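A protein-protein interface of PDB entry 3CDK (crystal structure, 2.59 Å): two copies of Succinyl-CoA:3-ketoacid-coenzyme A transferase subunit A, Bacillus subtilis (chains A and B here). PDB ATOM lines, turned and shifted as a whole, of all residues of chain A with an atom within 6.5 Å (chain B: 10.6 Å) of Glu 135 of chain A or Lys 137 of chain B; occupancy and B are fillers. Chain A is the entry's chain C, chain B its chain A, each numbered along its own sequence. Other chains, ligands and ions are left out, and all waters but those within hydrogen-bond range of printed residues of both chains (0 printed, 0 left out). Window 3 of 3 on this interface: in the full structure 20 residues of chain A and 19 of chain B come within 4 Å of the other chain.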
ATOM      1  N   TYR A 121       5.337   0.630 -21.423  1.00  0.00           N
ATOM      2  CA  TYR A 121       5.979  -0.717 -21.323  1.00  0.00           C
ATOM      3  C   TYR A 121       5.079  -1.782 -21.928  1.00  0.00           C
ATOM      4  O   TYR A 121       3.835  -1.687 -21.854  1.00  0.00           O
ATOM      5  CB  TYR A 121       6.353  -1.099 -19.847  1.00  0.00           C
ATOM      6  CG  TYR A 121       7.525  -0.326 -19.365  1.00  0.00           C
ATOM      7  CD1 TYR A 121       8.817  -0.795 -19.567  1.00  0.00           C
ATOM      8  CD2 TYR A 121       7.358   0.911 -18.756  1.00  0.00           C
ATOM      9  CE1 TYR A 121       9.914  -0.078 -19.150  1.00  0.00           C
ATOM     10  CE2 TYR A 121       8.455   1.661 -18.326  1.00  0.00           C
ATOM     11  CZ  TYR A 121       9.732   1.162 -18.546  1.00  0.00           C
ATOM     12  OH  TYR A 121      10.828   1.888 -18.138  1.00  0.00           O
ATOM     13  N   ALA A 131      14.059  -6.291 -28.942  1.00  0.00           N
ATOM     14  CA  ALA A 131      14.235  -5.618 -27.673  1.00  0.00           C
ATOM     15  C   ALA A 131      15.691  -5.248 -27.386  1.00  0.00           C
ATOM     16  O   ALA A 131      15.954  -4.591 -26.389  1.00  0.00           O
ATOM     17  CB  ALA A 131      13.667  -6.462 -26.549  1.00  0.00           C
ATOM     18  N   GLY A 133      18.966  -3.162 -27.090  1.00  0.00           N
ATOM     19  CA  GLY A 133      19.219  -1.715 -26.970  1.00  0.00           C
ATOM     20  C   GLY A 133      18.185  -0.824 -26.255  1.00  0.00           C
ATOM     21  O   GLY A 133      18.334   0.424 -26.236  1.00  0.00           O
ATOM     22  N   LYS A 134      17.149  -1.435 -25.665  1.00  0.00           N
ATOM     23  CA  LYS A 134      16.097  -0.678 -24.975  1.00  0.00           C
ATOM     24  C   LYS A 134      15.983  -1.004 -23.486  1.00  0.00           C
ATOM     25  O   LYS A 134      16.295  -2.108 -23.075  1.00  0.00           O
ATOM     26  CB  LYS A 134      14.749  -0.947 -25.610  1.00  0.00           C
ATOM     27  CG  LYS A 134      14.670  -0.699 -27.101  1.00  0.00           C
ATOM     28  CD  LYS A 134      13.387  -1.325 -27.635  1.00  0.00           C
ATOM     29  CE  LYS A 134      13.140  -0.962 -29.086  1.00  0.00           C
ATOM     30  NZ  LYS A 134      12.128  -1.899 -29.599  1.00  0.00           N
ATOM     31  N   GLU A 135      15.499  -0.048 -22.688  1.00  0.00           N
ATOM     32  CA  GLU A 135      15.312  -0.265 -21.266  1.00  0.00           C
ATOM     33  C   GLU A 135      14.380  -1.454 -20.990  1.00  0.00           C
ATOM     34  O   GLU A 135      13.333  -1.613 -21.623  1.00  0.00           O
ATOM     35  CB  GLU A 135      14.774   0.993 -20.592  1.00  0.00           C
ATOM     36  CG  GLU A 135      15.743   2.134 -20.484  1.00  0.00           C
ATOM     37  CD  GLU A 135      15.658   3.083 -21.669  1.00  0.00           C
ATOM     38  OE1 GLU A 135      15.193   2.654 -22.765  1.00  0.00           O
ATOM     39  OE2 GLU A 135      16.050   4.266 -21.518  1.00  0.00           O
ATOM     40  N   HIS A 136      14.777  -2.274 -20.029  1.00  0.00           N
ATOM     41  CA  HIS A 136      13.984  -3.398 -19.555  1.00  0.00           C
ATOM     42  C   HIS A 136      13.558  -3.123 -18.121  1.00  0.00           C
ATOM     43  O   HIS A 136      14.328  -2.618 -17.304  1.00  0.00           O
ATOM     44  CB  HIS A 136      14.820  -4.672 -19.610  1.00  0.00           C
ATOM     45  CG  HIS A 136      14.959  -5.236 -20.987  1.00  0.00           C
ATOM     46  ND1 HIS A 136      15.362  -4.479 -22.069  1.00  0.00           N
ATOM     47  CD2 HIS A 136      14.766  -6.490 -21.460  1.00  0.00           C
ATOM     48  CE1 HIS A 136      15.393  -5.237 -23.150  1.00  0.00           C
ATOM     49  NE2 HIS A 136      15.037  -6.462 -22.808  1.00  0.00           N
ATOM     50  N   LYS A 137      12.324  -3.459 -17.814  1.00  0.00           N
ATOM     51  CA  LYS A 137      11.805  -3.249 -16.468  1.00  0.00           C
ATOM     52  C   LYS A 137      10.877  -4.403 -16.105  1.00  0.00           C
ATOM     53  O   LYS A 137      10.111  -4.906 -16.944  1.00  0.00           O
ATOM     54  CB  LYS A 137      11.076  -1.918 -16.391  1.00  0.00           C
ATOM     55  CG  LYS A 137      10.745  -1.445 -14.985  1.00  0.00           C
ATOM     56  CD  LYS A 137      10.298   0.016 -15.000  1.00  0.00           C
ATOM     57  CE  LYS A 137       9.749   0.425 -13.645  1.00  0.00           C
ATOM     58  NZ  LYS A 137      10.789   0.413 -12.532  1.00  0.00           N
ATOM     59  N   TYR A 144       9.429  -6.395 -19.195  1.00  0.00           N
ATOM     60  CA  TYR A 144       8.851  -5.546 -20.247  1.00  0.00           C
ATOM     61  C   TYR A 144       9.923  -4.637 -20.897  1.00  0.00           C
ATOM     62  O   TYR A 144      11.007  -4.391 -20.301  1.00  0.00           O
ATOM     63  CB  TYR A 144       7.698  -4.714 -19.673  1.00  0.00           C
ATOM     64  CG  TYR A 144       6.558  -5.569 -19.112  1.00  0.00           C
ATOM     65  CD1 TYR A 144       6.620  -6.089 -17.807  1.00  0.00           C
ATOM     66  CD2 TYR A 144       5.437  -5.902 -19.899  1.00  0.00           C
ATOM     67  CE1 TYR A 144       5.597  -6.903 -17.306  1.00  0.00           C
ATOM     68  CE2 TYR A 144       4.404  -6.707 -19.390  1.00  0.00           C
ATOM     69  CZ  TYR A 144       4.503  -7.183 -18.097  1.00  0.00           C
ATOM     70  OH  TYR A 144       3.516  -7.948 -17.581  1.00  0.00           O
ATOM     71  N   VAL A 145       9.662  -4.203 -22.131  1.00  0.00           N
ATOM     72  CA  VAL A 145      10.534  -3.251 -22.811  1.00  0.00           C
ATOM     73  C   VAL A 145       9.890  -1.881 -22.852  1.00  0.00           C
ATOM     74  O   VAL A 145       8.709  -1.773 -23.117  1.00  0.00           O
ATOM     75  CB  VAL A 145      10.748  -3.578 -24.307  1.00  0.00           C
ATOM     76  CG1 VAL A 145      12.144  -3.150 -24.727  1.00  0.00           C
ATOM     77  CG2 VAL A 145      10.493  -5.034 -24.616  1.00  0.00           C
ATOM     78  N   LEU A 146      10.687  -0.838 -22.642  1.00  0.00           N
ATOM     79  CA  LEU A 146      10.206   0.526 -22.860  1.00  0.00           C
ATOM     80  C   LEU A 146      10.079   0.798 -24.343  1.00  0.00           C
ATOM     81  O   LEU A 146      11.072   0.671 -25.085  1.00  0.00           O
ATOM     82  CB  LEU A 146      11.190   1.510 -22.246  1.00  0.00           C
ATOM     83  CG  LEU A 146      10.950   3.006 -22.381  1.00  0.00           C
ATOM     84  CD1 LEU A 146       9.601   3.330 -21.836  1.00  0.00           C
ATOM     85  CD2 LEU A 146      12.034   3.765 -21.632  1.00  0.00           C
ATOM     86  N   GLU A 147       8.881   1.174 -24.791  1.00  0.00           N
ATOM     87  CA  GLU A 147       8.723   1.700 -26.141  1.00  0.00           C
ATOM     88  C   GLU A 147       8.357   3.203 -26.144  1.00  0.00           C
ATOM     89  O   GLU A 147       7.576   3.678 -25.305  1.00  0.00           O
ATOM     90  CB  GLU A 147       7.728   0.845 -26.915  1.00  0.00           C
ATOM     91  CG  GLU A 147       8.173  -0.626 -27.096  1.00  0.00           C
ATOM     92  CD  GLU A 147       9.267  -0.879 -28.226  1.00  0.00           C
ATOM     93  OE1 GLU A 147       9.645   0.022 -29.016  1.00  0.00           O
ATOM     94  OE2 GLU A 147       9.745  -2.028 -28.347  1.00  0.00           O
ATOM     95  N   ARG A 148       8.924   3.937 -27.099  1.00  0.00           N
ATOM     96  CA  ARG A 148       8.778   5.401 -27.195  1.00  0.00           C
ATOM     97  C   ARG A 148       7.710   5.942 -28.132  1.00  0.00           C
ATOM     98  O   ARG A 148       7.558   5.483 -29.293  1.00  0.00           O
ATOM     99  CB  ARG A 148      10.135   6.023 -27.502  1.00  0.00           C
ATOM    100  CG  ARG A 148      11.053   5.868 -26.273  1.00  0.00           C
ATOM    101  CD  ARG A 148      12.483   6.283 -26.469  1.00  0.00           C
ATOM    102  NE  ARG A 148      13.280   5.560 -25.496  1.00  0.00           N
ATOM    103  CZ  ARG A 148      13.996   6.114 -24.532  1.00  0.00           C
ATOM    104  NH1 ARG A 148      14.105   7.433 -24.432  1.00  0.00           N
ATOM    105  NH2 ARG A 148      14.649   5.336 -23.688  1.00  0.00           N
ATOM    106  N   PRO B 118       1.721  -2.431 -18.436  1.00  0.00           N
ATOM    107  CA  PRO B 118       1.921  -2.354 -16.987  1.00  0.00           C
ATOM    108  C   PRO B 118       2.207  -0.947 -16.469  1.00  0.00           C
ATOM    109  O   PRO B 118       1.927  -0.659 -15.280  1.00  0.00           O
ATOM    110  CB  PRO B 118       3.115  -3.261 -16.732  1.00  0.00           C
ATOM    111  CG  PRO B 118       3.839  -3.362 -18.074  1.00  0.00           C
ATOM    112  CD  PRO B 118       2.792  -3.180 -19.125  1.00  0.00           C
ATOM    113  N   GLY B 119       2.743  -0.072 -17.336  1.00  0.00           N
ATOM    114  CA  GLY B 119       3.132   1.265 -16.917  1.00  0.00           C
ATOM    115  C   GLY B 119       3.329   2.176 -18.109  1.00  0.00           C
ATOM    116  O   GLY B 119       3.602   1.701 -19.180  1.00  0.00           O
ATOM    117  N   PHE B 120       3.215   3.489 -17.914  1.00  0.00           N
ATOM    118  CA  PHE B 120       3.487   4.462 -18.965  1.00  0.00           C
ATOM    119  C   PHE B 120       3.811   5.782 -18.279  1.00  0.00           C
ATOM    120  O   PHE B 120       3.456   5.991 -17.122  1.00  0.00           O
ATOM    121  CB  PHE B 120       2.259   4.667 -19.884  1.00  0.00           C
ATOM    122  CG  PHE B 120       1.077   5.239 -19.160  1.00  0.00           C
ATOM    123  CD1 PHE B 120       0.274   4.420 -18.358  1.00  0.00           C
ATOM    124  CD2 PHE B 120       0.836   6.601 -19.175  1.00  0.00           C
ATOM    125  CE1 PHE B 120      -0.802   4.964 -17.627  1.00  0.00           C
ATOM    126  CE2 PHE B 120      -0.220   7.171 -18.431  1.00  0.00           C
ATOM    127  CZ  PHE B 120      -1.047   6.361 -17.662  1.00  0.00           C
ATOM    128  N   TYR B 121       4.418   6.697 -19.015  1.00  0.00           N
ATOM    129  CA  TYR B 121       4.932   7.917 -18.439  1.00  0.00           C
ATOM    130  C   TYR B 121       4.039   9.038 -18.784  1.00  0.00           C
ATOM    131  O   TYR B 121       3.476   9.053 -19.888  1.00  0.00           O
ATOM    132  CB  TYR B 121       6.304   8.205 -19.010  1.00  0.00           C
ATOM    133  CG  TYR B 121       7.339   7.543 -18.214  1.00  0.00           C
ATOM    134  CD1 TYR B 121       7.727   8.075 -16.994  1.00  0.00           C
ATOM    135  CD2 TYR B 121       7.905   6.344 -18.630  1.00  0.00           C
ATOM    136  CE1 TYR B 121       8.686   7.437 -16.216  1.00  0.00           C
ATOM    137  CE2 TYR B 121       8.873   5.709 -17.874  1.00  0.00           C
ATOM    138  CZ  TYR B 121       9.255   6.272 -16.674  1.00  0.00           C
ATOM    139  OH  TYR B 121      10.202   5.681 -15.901  1.00  0.00           O
ATOM    140  N   THR B 122       3.903   9.986 -17.876  1.00  0.00           N
ATOM    141  CA  THR B 122       3.128  11.165 -18.160  1.00  0.00           C
ATOM    142  C   THR B 122       3.738  12.345 -17.380  1.00  0.00           C
ATOM    143  O   THR B 122       4.428  12.137 -16.368  1.00  0.00           O
ATOM    144  CB  THR B 122       1.632  10.928 -17.802  1.00  0.00           C
ATOM    145  OG1 THR B 122       0.870  12.129 -18.006  1.00  0.00           O
ATOM    146  CG2 THR B 122       1.496  10.533 -16.354  1.00  0.00           C
ATOM    147  N   ALA B 123       3.475  13.557 -17.860  1.00  0.00           N
ATOM    148  CA  ALA B 123       3.885  14.809 -17.214  1.00  0.00           C
ATOM    149  C   ALA B 123       2.896  15.232 -16.119  1.00  0.00           C
ATOM    150  O   ALA B 123       3.229  16.028 -15.247  1.00  0.00           O
ATOM    151  CB  ALA B 123       3.973  15.903 -18.257  1.00  0.00           C
ATOM    152  N   THR B 124       1.666  14.735 -16.197  1.00  0.00           N
ATOM    153  CA  THR B 124       0.650  15.082 -15.238  1.00  0.00           C
ATOM    154  C   THR B 124       1.077  14.753 -13.827  1.00  0.00           C
ATOM    155  O   THR B 124       1.423  13.616 -13.530  1.00  0.00           O
ATOM    156  CB  THR B 124      -0.610  14.336 -15.551  1.00  0.00           C
ATOM    157  OG1 THR B 124      -1.010  14.683 -16.879  1.00  0.00           O
ATOM    158  CG2 THR B 124      -1.694  14.701 -14.558  1.00  0.00           C
ATOM    159  N   VAL B 126       3.828  15.791 -12.167  1.00  0.00           N
ATOM    160  CA  VAL B 126       5.225  16.087 -11.883  1.00  0.00           C
ATOM    161  C   VAL B 126       5.339  17.309 -10.940  1.00  0.00           C
ATOM    162  O   VAL B 126       4.544  18.247 -11.044  1.00  0.00           O
ATOM    163  CB  VAL B 126       6.091  16.221 -13.218  1.00  0.00           C
ATOM    164  CG1 VAL B 126       7.527  16.776 -12.937  1.00  0.00           C
ATOM    165  CG2 VAL B 126       6.146  14.849 -13.980  1.00  0.00           C
ATOM    166  N   GLY B 127       6.312  17.252 -10.008  1.00  0.00           N
ATOM    167  CA  GLY B 127       6.528  18.294  -8.961  1.00  0.00           C
ATOM    168  C   GLY B 127       5.371  18.506  -7.970  1.00  0.00           C
ATOM    169  O   GLY B 127       5.262  19.549  -7.329  1.00  0.00           O
ATOM    170  N   ALA B 131       3.462  12.713  -7.595  1.00  0.00           N
ATOM    171  CA  ALA B 131       4.750  12.178  -8.061  1.00  0.00           C
ATOM    172  C   ALA B 131       5.439  11.278  -7.029  1.00  0.00           C
ATOM    173  O   ALA B 131       6.391  10.554  -7.363  1.00  0.00           O
ATOM    174  CB  ALA B 131       5.687  13.344  -8.416  1.00  0.00           C
ATOM    175  N   GLY B 133       6.972   8.588  -4.759  1.00  0.00           N
ATOM    176  CA  GLY B 133       7.253   7.151  -4.964  1.00  0.00           C
ATOM    177  C   GLY B 133       7.083   6.631  -6.391  1.00  0.00           C
ATOM    178  O   GLY B 133       7.073   5.412  -6.620  1.00  0.00           O
ATOM    179  N   LYS B 134       6.897   7.512  -7.357  1.00  0.00           N
ATOM    180  CA  LYS B 134       6.824   7.038  -8.742  1.00  0.00           C
ATOM    181  C   LYS B 134       8.182   7.232  -9.450  1.00  0.00           C
ATOM    182  O   LYS B 134       8.973   8.091  -9.074  1.00  0.00           O
ATOM    183  CB  LYS B 134       5.641   7.688  -9.505  1.00  0.00           C
ATOM    184  CG  LYS B 134       4.394   7.645  -8.657  1.00  0.00           C
ATOM    185  CD  LYS B 134       3.088   7.876  -9.413  1.00  0.00           C
ATOM    186  CE  LYS B 134       1.903   7.417  -8.554  1.00  0.00           C
ATOM    187  NZ  LYS B 134       0.701   8.234  -8.867  1.00  0.00           N
ATOM    188  N   GLU B 135       8.457   6.414 -10.445  1.00  0.00           N
ATOM    189  CA  GLU B 135       9.665   6.601 -11.263  1.00  0.00           C
ATOM    190  C   GLU B 135       9.612   7.904 -12.023  1.00  0.00           C
ATOM    191  O   GLU B 135       8.578   8.242 -12.597  1.00  0.00           O
ATOM    192  CB  GLU B 135       9.854   5.447 -12.238  1.00  0.00           C
ATOM    193  CG  GLU B 135      10.185   4.168 -11.533  1.00  0.00           C
ATOM    194  CD  GLU B 135       8.981   3.331 -11.148  1.00  0.00           C
ATOM    195  OE1 GLU B 135       7.826   3.833 -11.058  1.00  0.00           O
ATOM    196  OE2 GLU B 135       9.207   2.130 -10.939  1.00  0.00           O
ATOM    197  N   HIS B 136      10.721   8.639 -11.979  1.00  0.00           N
ATOM    198  CA  HIS B 136      10.856   9.865 -12.743  1.00  0.00           C
ATOM    199  C   HIS B 136      11.848   9.578 -13.879  1.00  0.00           C
ATOM    200  O   HIS B 136      12.889   8.981 -13.656  1.00  0.00           O
ATOM    201  CB  HIS B 136      11.345  11.025 -11.867  1.00  0.00           C
ATOM    202  CG  HIS B 136      10.314  11.584 -10.917  1.00  0.00           C
ATOM    203  ND1 HIS B 136       9.677  10.821  -9.956  1.00  0.00           N
ATOM    204  CD2 HIS B 136       9.863  12.854 -10.737  1.00  0.00           C
ATOM    205  CE1 HIS B 136       8.868  11.592  -9.246  1.00  0.00           C
ATOM    206  NE2 HIS B 136       8.962  12.830  -9.699  1.00  0.00           N
ATOM    207  N   LYS B 137      11.508   9.974 -15.104  1.00  0.00           N
ATOM    208  CA  LYS B 137      12.419   9.796 -16.247  1.00  0.00           C
ATOM    209  C   LYS B 137      12.349  11.012 -17.175  1.00  0.00           C
ATOM    210  O   LYS B 137      11.264  11.581 -17.347  1.00  0.00           O
ATOM    211  CB  LYS B 137      12.057   8.511 -17.008  1.00  0.00           C
ATOM    212  CG  LYS B 137      13.102   8.063 -17.991  1.00  0.00           C
ATOM    213  CD  LYS B 137      12.866   6.638 -18.477  1.00  0.00           C
ATOM    214  CE  LYS B 137      13.625   6.378 -19.776  1.00  0.00           C
ATOM    215  NZ  LYS B 137      15.116   6.545 -19.628  1.00  0.00           N
ATOM    216  N   THR B 138      13.483  11.367 -17.785  1.00  0.00           N
ATOM    217  CA  THR B 138      13.623  12.507 -18.709  1.00  0.00           C
ATOM    218  C   THR B 138      13.438  12.079 -20.155  1.00  0.00           C
ATOM    219  O   THR B 138      14.072  11.140 -20.614  1.00  0.00           O
ATOM    220  CB  THR B 138      15.038  13.133 -18.616  1.00  0.00           C
ATOM    221  OG1 THR B 138      15.401  13.334 -17.247  1.00  0.00           O
ATOM    222  CG2 THR B 138      15.125  14.468 -19.371  1.00  0.00           C
ATOM    223  N   PHE B 139      12.553  12.769 -20.868  1.00  0.00           N
ATOM    224  CA  PHE B 139      12.341  12.558 -22.303  1.00  0.00           C
ATOM    225  C   PHE B 139      12.378  13.907 -22.997  1.00  0.00           C
ATOM    226  O   PHE B 139      11.722  14.841 -22.573  1.00  0.00           O
ATOM    227  CB  PHE B 139      11.005  11.885 -22.583  1.00  0.00           C
ATOM    228  CG  PHE B 139      10.885  10.459 -22.052  1.00  0.00           C
ATOM    229  CD1 PHE B 139      11.197   9.374 -22.859  1.00  0.00           C
ATOM    230  CD2 PHE B 139      10.377  10.211 -20.768  1.00  0.00           C
ATOM    231  CE1 PHE B 139      11.047   8.055 -22.402  1.00  0.00           C
ATOM    232  CE2 PHE B 139      10.219   8.888 -20.276  1.00  0.00           C
ATOM    233  CZ  PHE B 139      10.564   7.803 -21.098  1.00  0.00           C
ATOM    234  N   GLY B 140      13.186  14.023 -24.039  1.00  0.00           N
ATOM    235  CA  GLY B 140      13.418  15.319 -24.664  1.00  0.00           C
ATOM    236  C   GLY B 140      13.552  16.450 -23.662  1.00  0.00           C
ATOM    237  O   GLY B 140      12.804  17.406 -23.717  1.00  0.00           O
ATOM    238  N   GLY B 141      14.481  16.322 -22.718  1.00  0.00           N
ATOM    239  CA  GLY B 141      14.745  17.393 -21.737  1.00  0.00           C
ATOM    240  C   GLY B 141      13.670  17.740 -20.707  1.00  0.00           C
ATOM    241  O   GLY B 141      13.822  18.706 -19.987  1.00  0.00           O
ATOM    242  N   ARG B 142      12.598  16.948 -20.612  1.00  0.00           N
ATOM    243  CA  ARG B 142      11.551  17.206 -19.630  1.00  0.00           C
ATOM    244  C   ARG B 142      11.193  15.959 -18.777  1.00  0.00           C
ATOM    245  O   ARG B 142      11.293  14.826 -19.240  1.00  0.00           O
ATOM    246  CB  ARG B 142      10.337  17.828 -20.353  1.00  0.00           C
ATOM    247  CG  ARG B 142       8.942  17.410 -19.861  1.00  0.00           C
ATOM    248  CD  ARG B 142       7.839  17.936 -20.851  1.00  0.00           C
ATOM    249  NE  ARG B 142       6.628  18.530 -20.246  1.00  0.00           N
ATOM    250  CZ  ARG B 142       5.370  18.302 -20.663  1.00  0.00           C
ATOM    251  NH1 ARG B 142       5.127  17.441 -21.651  1.00  0.00           N
ATOM    252  NH2 ARG B 142       4.330  18.918 -20.072  1.00  0.00           N
ATOM    253  N   THR B 143      10.784  16.203 -17.528  1.00  0.00           N
ATOM    254  CA  THR B 143      10.452  15.164 -16.559  1.00  0.00           C
ATOM    255  C   THR B 143       9.025  14.542 -16.678  1.00  0.00           C
ATOM    256  O   THR B 143       8.022  15.257 -16.752  1.00  0.00           O
ATOM    257  CB  THR B 143      10.700  15.667 -15.108  1.00  0.00           C
ATOM    258  OG1 THR B 143      12.080  16.035 -14.957  1.00  0.00           O
ATOM    259  CG2 THR B 143      10.401  14.609 -14.116  1.00  0.00           C
ATOM    260  N   TYR B 144       8.970  13.208 -16.664  1.00  0.00           N
ATOM    261  CA  TYR B 144       7.735  12.493 -16.587  1.00  0.00           C
ATOM    262  C   TYR B 144       7.815  11.508 -15.447  1.00  0.00           C
ATOM    263  O   TYR B 144       8.926  11.071 -15.048  1.00  0.00           O
ATOM    264  CB  TYR B 144       7.406  11.758 -17.894  1.00  0.00           C
ATOM    265  CG  TYR B 144       7.415  12.691 -19.080  1.00  0.00           C
ATOM    266  CD1 TYR B 144       8.617  13.059 -19.690  1.00  0.00           C
ATOM    267  CD2 TYR B 144       6.227  13.225 -19.586  1.00  0.00           C
ATOM    268  CE1 TYR B 144       8.633  13.902 -20.740  1.00  0.00           C
ATOM    269  CE2 TYR B 144       6.237  14.082 -20.669  1.00  0.00           C
ATOM    270  CZ  TYR B 144       7.455  14.416 -21.231  1.00  0.00           C
ATOM    271  OH  TYR B 144       7.516  15.270 -22.314  1.00  0.00           O
ATOM    272  N   VAL B 145       6.623  11.133 -14.975  1.00  0.00           N
ATOM    273  CA  VAL B 145       6.444  10.194 -13.892  1.00  0.00           C
ATOM    274  C   VAL B 145       5.797   8.901 -14.419  1.00  0.00           C
ATOM    275  O   VAL B 145       4.932   8.964 -15.323  1.00  0.00           O
ATOM    276  CB  VAL B 145       5.614  10.903 -12.751  1.00  0.00           C
ATOM    277  CG1 VAL B 145       4.101  10.954 -13.026  1.00  0.00           C
ATOM    278  CG2 VAL B 145       5.837  10.254 -11.478  1.00  0.00           C
ATOM    279  N   LEU B 146       6.200   7.744 -13.892  1.00  0.00           N
ATOM    280  CA  LEU B 146       5.556   6.430 -14.293  1.00  0.00           C
ATOM    281  C   LEU B 146       4.256   6.113 -13.557  1.00  0.00           C
ATOM    282  O   LEU B 146       4.188   6.178 -12.316  1.00  0.00           O
ATOM    283  CB  LEU B 146       6.504   5.242 -14.141  1.00  0.00           C
ATOM    284  CG  LEU B 146       6.025   3.862 -14.687  1.00  0.00           C
ATOM    285  CD1 LEU B 146       6.049   3.796 -16.179  1.00  0.00           C
ATOM    286  CD2 LEU B 146       6.882   2.735 -14.221  1.00  0.00           C
ATOM    287  N   GLU B 147       3.225   5.787 -14.317  1.00  0.00           N
ATOM    288  CA  GLU B 147       1.916   5.404 -13.758  1.00  0.00           C
ATOM    289  C   GLU B 147       1.581   3.973 -14.171  1.00  0.00           C
ATOM    290  O   GLU B 147       1.884   3.559 -15.294  1.00  0.00           O
ATOM    291  CB  GLU B 147       0.821   6.384 -14.178  1.00  0.00           C
ATOM    292  CG  GLU B 147       0.934   7.796 -13.479  1.00  0.00           C
ATOM    293  CD  GLU B 147       0.695   7.818 -11.924  1.00  0.00           C
ATOM    294  OE1 GLU B 147       0.386   6.780 -11.294  1.00  0.00           O
ATOM    295  OE2 GLU B 147       0.857   8.898 -11.312  1.00  0.00           O
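Lys 137 of chain B touches just these residues of chain A: Glu 135 and Leu 146.
No residue of chain B comes within 4 Å of Gly 133 of chain A.
No residue of chain B comes within 4 Å of Val 145 of chain A.
Printed residues of chain B within 4 Å of Tyr 144 of chain A: Pro 118.
Of the printed residues of chain B, Tyr 121 of chain A touches Pro 118 (3.3 Å), Gly 119 (3.0 Å) and Leu 146 (3.9 Å).
The backbone NH (N) of Leu 146 of chain B sits at hydrogen-bond distance from the backbone carbonyl oxygen (O) of Glu 135 of chain B (2.8 Å).
The backbone NH (N) of Lys 137 of chain B is in hydrogen-bond range of the backbone carbonyl oxygen (O) of Tyr 144 of chain B (2.8 Å).
O of Glu 135 of chain A lies within hydrogen-bond range of N of Leu 146 of chain A (2.9 Å).
The side-chain carboxylate of Glu 135 of chain A lies within salt-bridge range of the guanidinium group of Arg 148 of chain A, at 2.8 Å.
The backbone NH (N) of Tyr 144 of chain A is in hydrogen-bond range of the backbone carbonyl oxygen (O) of Lys 137 of chain A.
Tyr 121 of chain A touches Leu 146 of chain B, but with the chains exchanged Leu 146 of chain A does not touch Tyr 121 of chain B (4.7 Å).
Glu 135 of chain A touches Lys 137 of chain B, and with the chains exchanged Lys 137 of chain A touches Glu 135 of chain B.
Lys 137 of chain A touches Leu 146 of chain B, and with the chains exchanged Leu 146 of chain A touches Lys 137 of chain B.
11 positions are printed for both chains.
Of the 9 pairs that touch across the chains among the printed residues, 4 have their exchanged pair printed and touching as well.
Of the 25 printed residues of chain B, 6 touch a printed residue of chain A.
Printed residues of chain B that touch a printed residue of chain A: Pro 118, Gly 119, Glu 135, Lys 137, Phe 139 and Leu 146.
Hydrophobic or aromatic side chains of chain A within 4 Å of the printed part of chain B: Tyr 121, Tyr 144 and Leu 146.
Tyr 121 of chain A touches Pro 118 of chain B (O to CD, 3.3 Å).
Tyr 121 of chain A touches Leu 146 of chain B.
Lys 137 of chain A touches Leu 146 of chain B (CE to CD2, 3.7 Å).
Tyr 144 of chain A touches Pro 118 of chain B.
Leu 146 of chain A touches Lys 137 of chain B (CD2 to CE, 3.6 Å).
Arg 148 of chain A touches Phe 139 of chain B.
N of Tyr 121 of chain A sits at hydrogen-bond distance from O of Gly 119 of chain B (3.0 Å).
The side-chain amino group (NZ) of Lys 137 of chain A is in salt-bridge range of the side-chain carboxylate (OE2) of Glu 135 of chain B (2.8 Å).
OE2 of Glu 135 of chain A is in salt-bridge range of NZ of Lys 137 of chain B.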
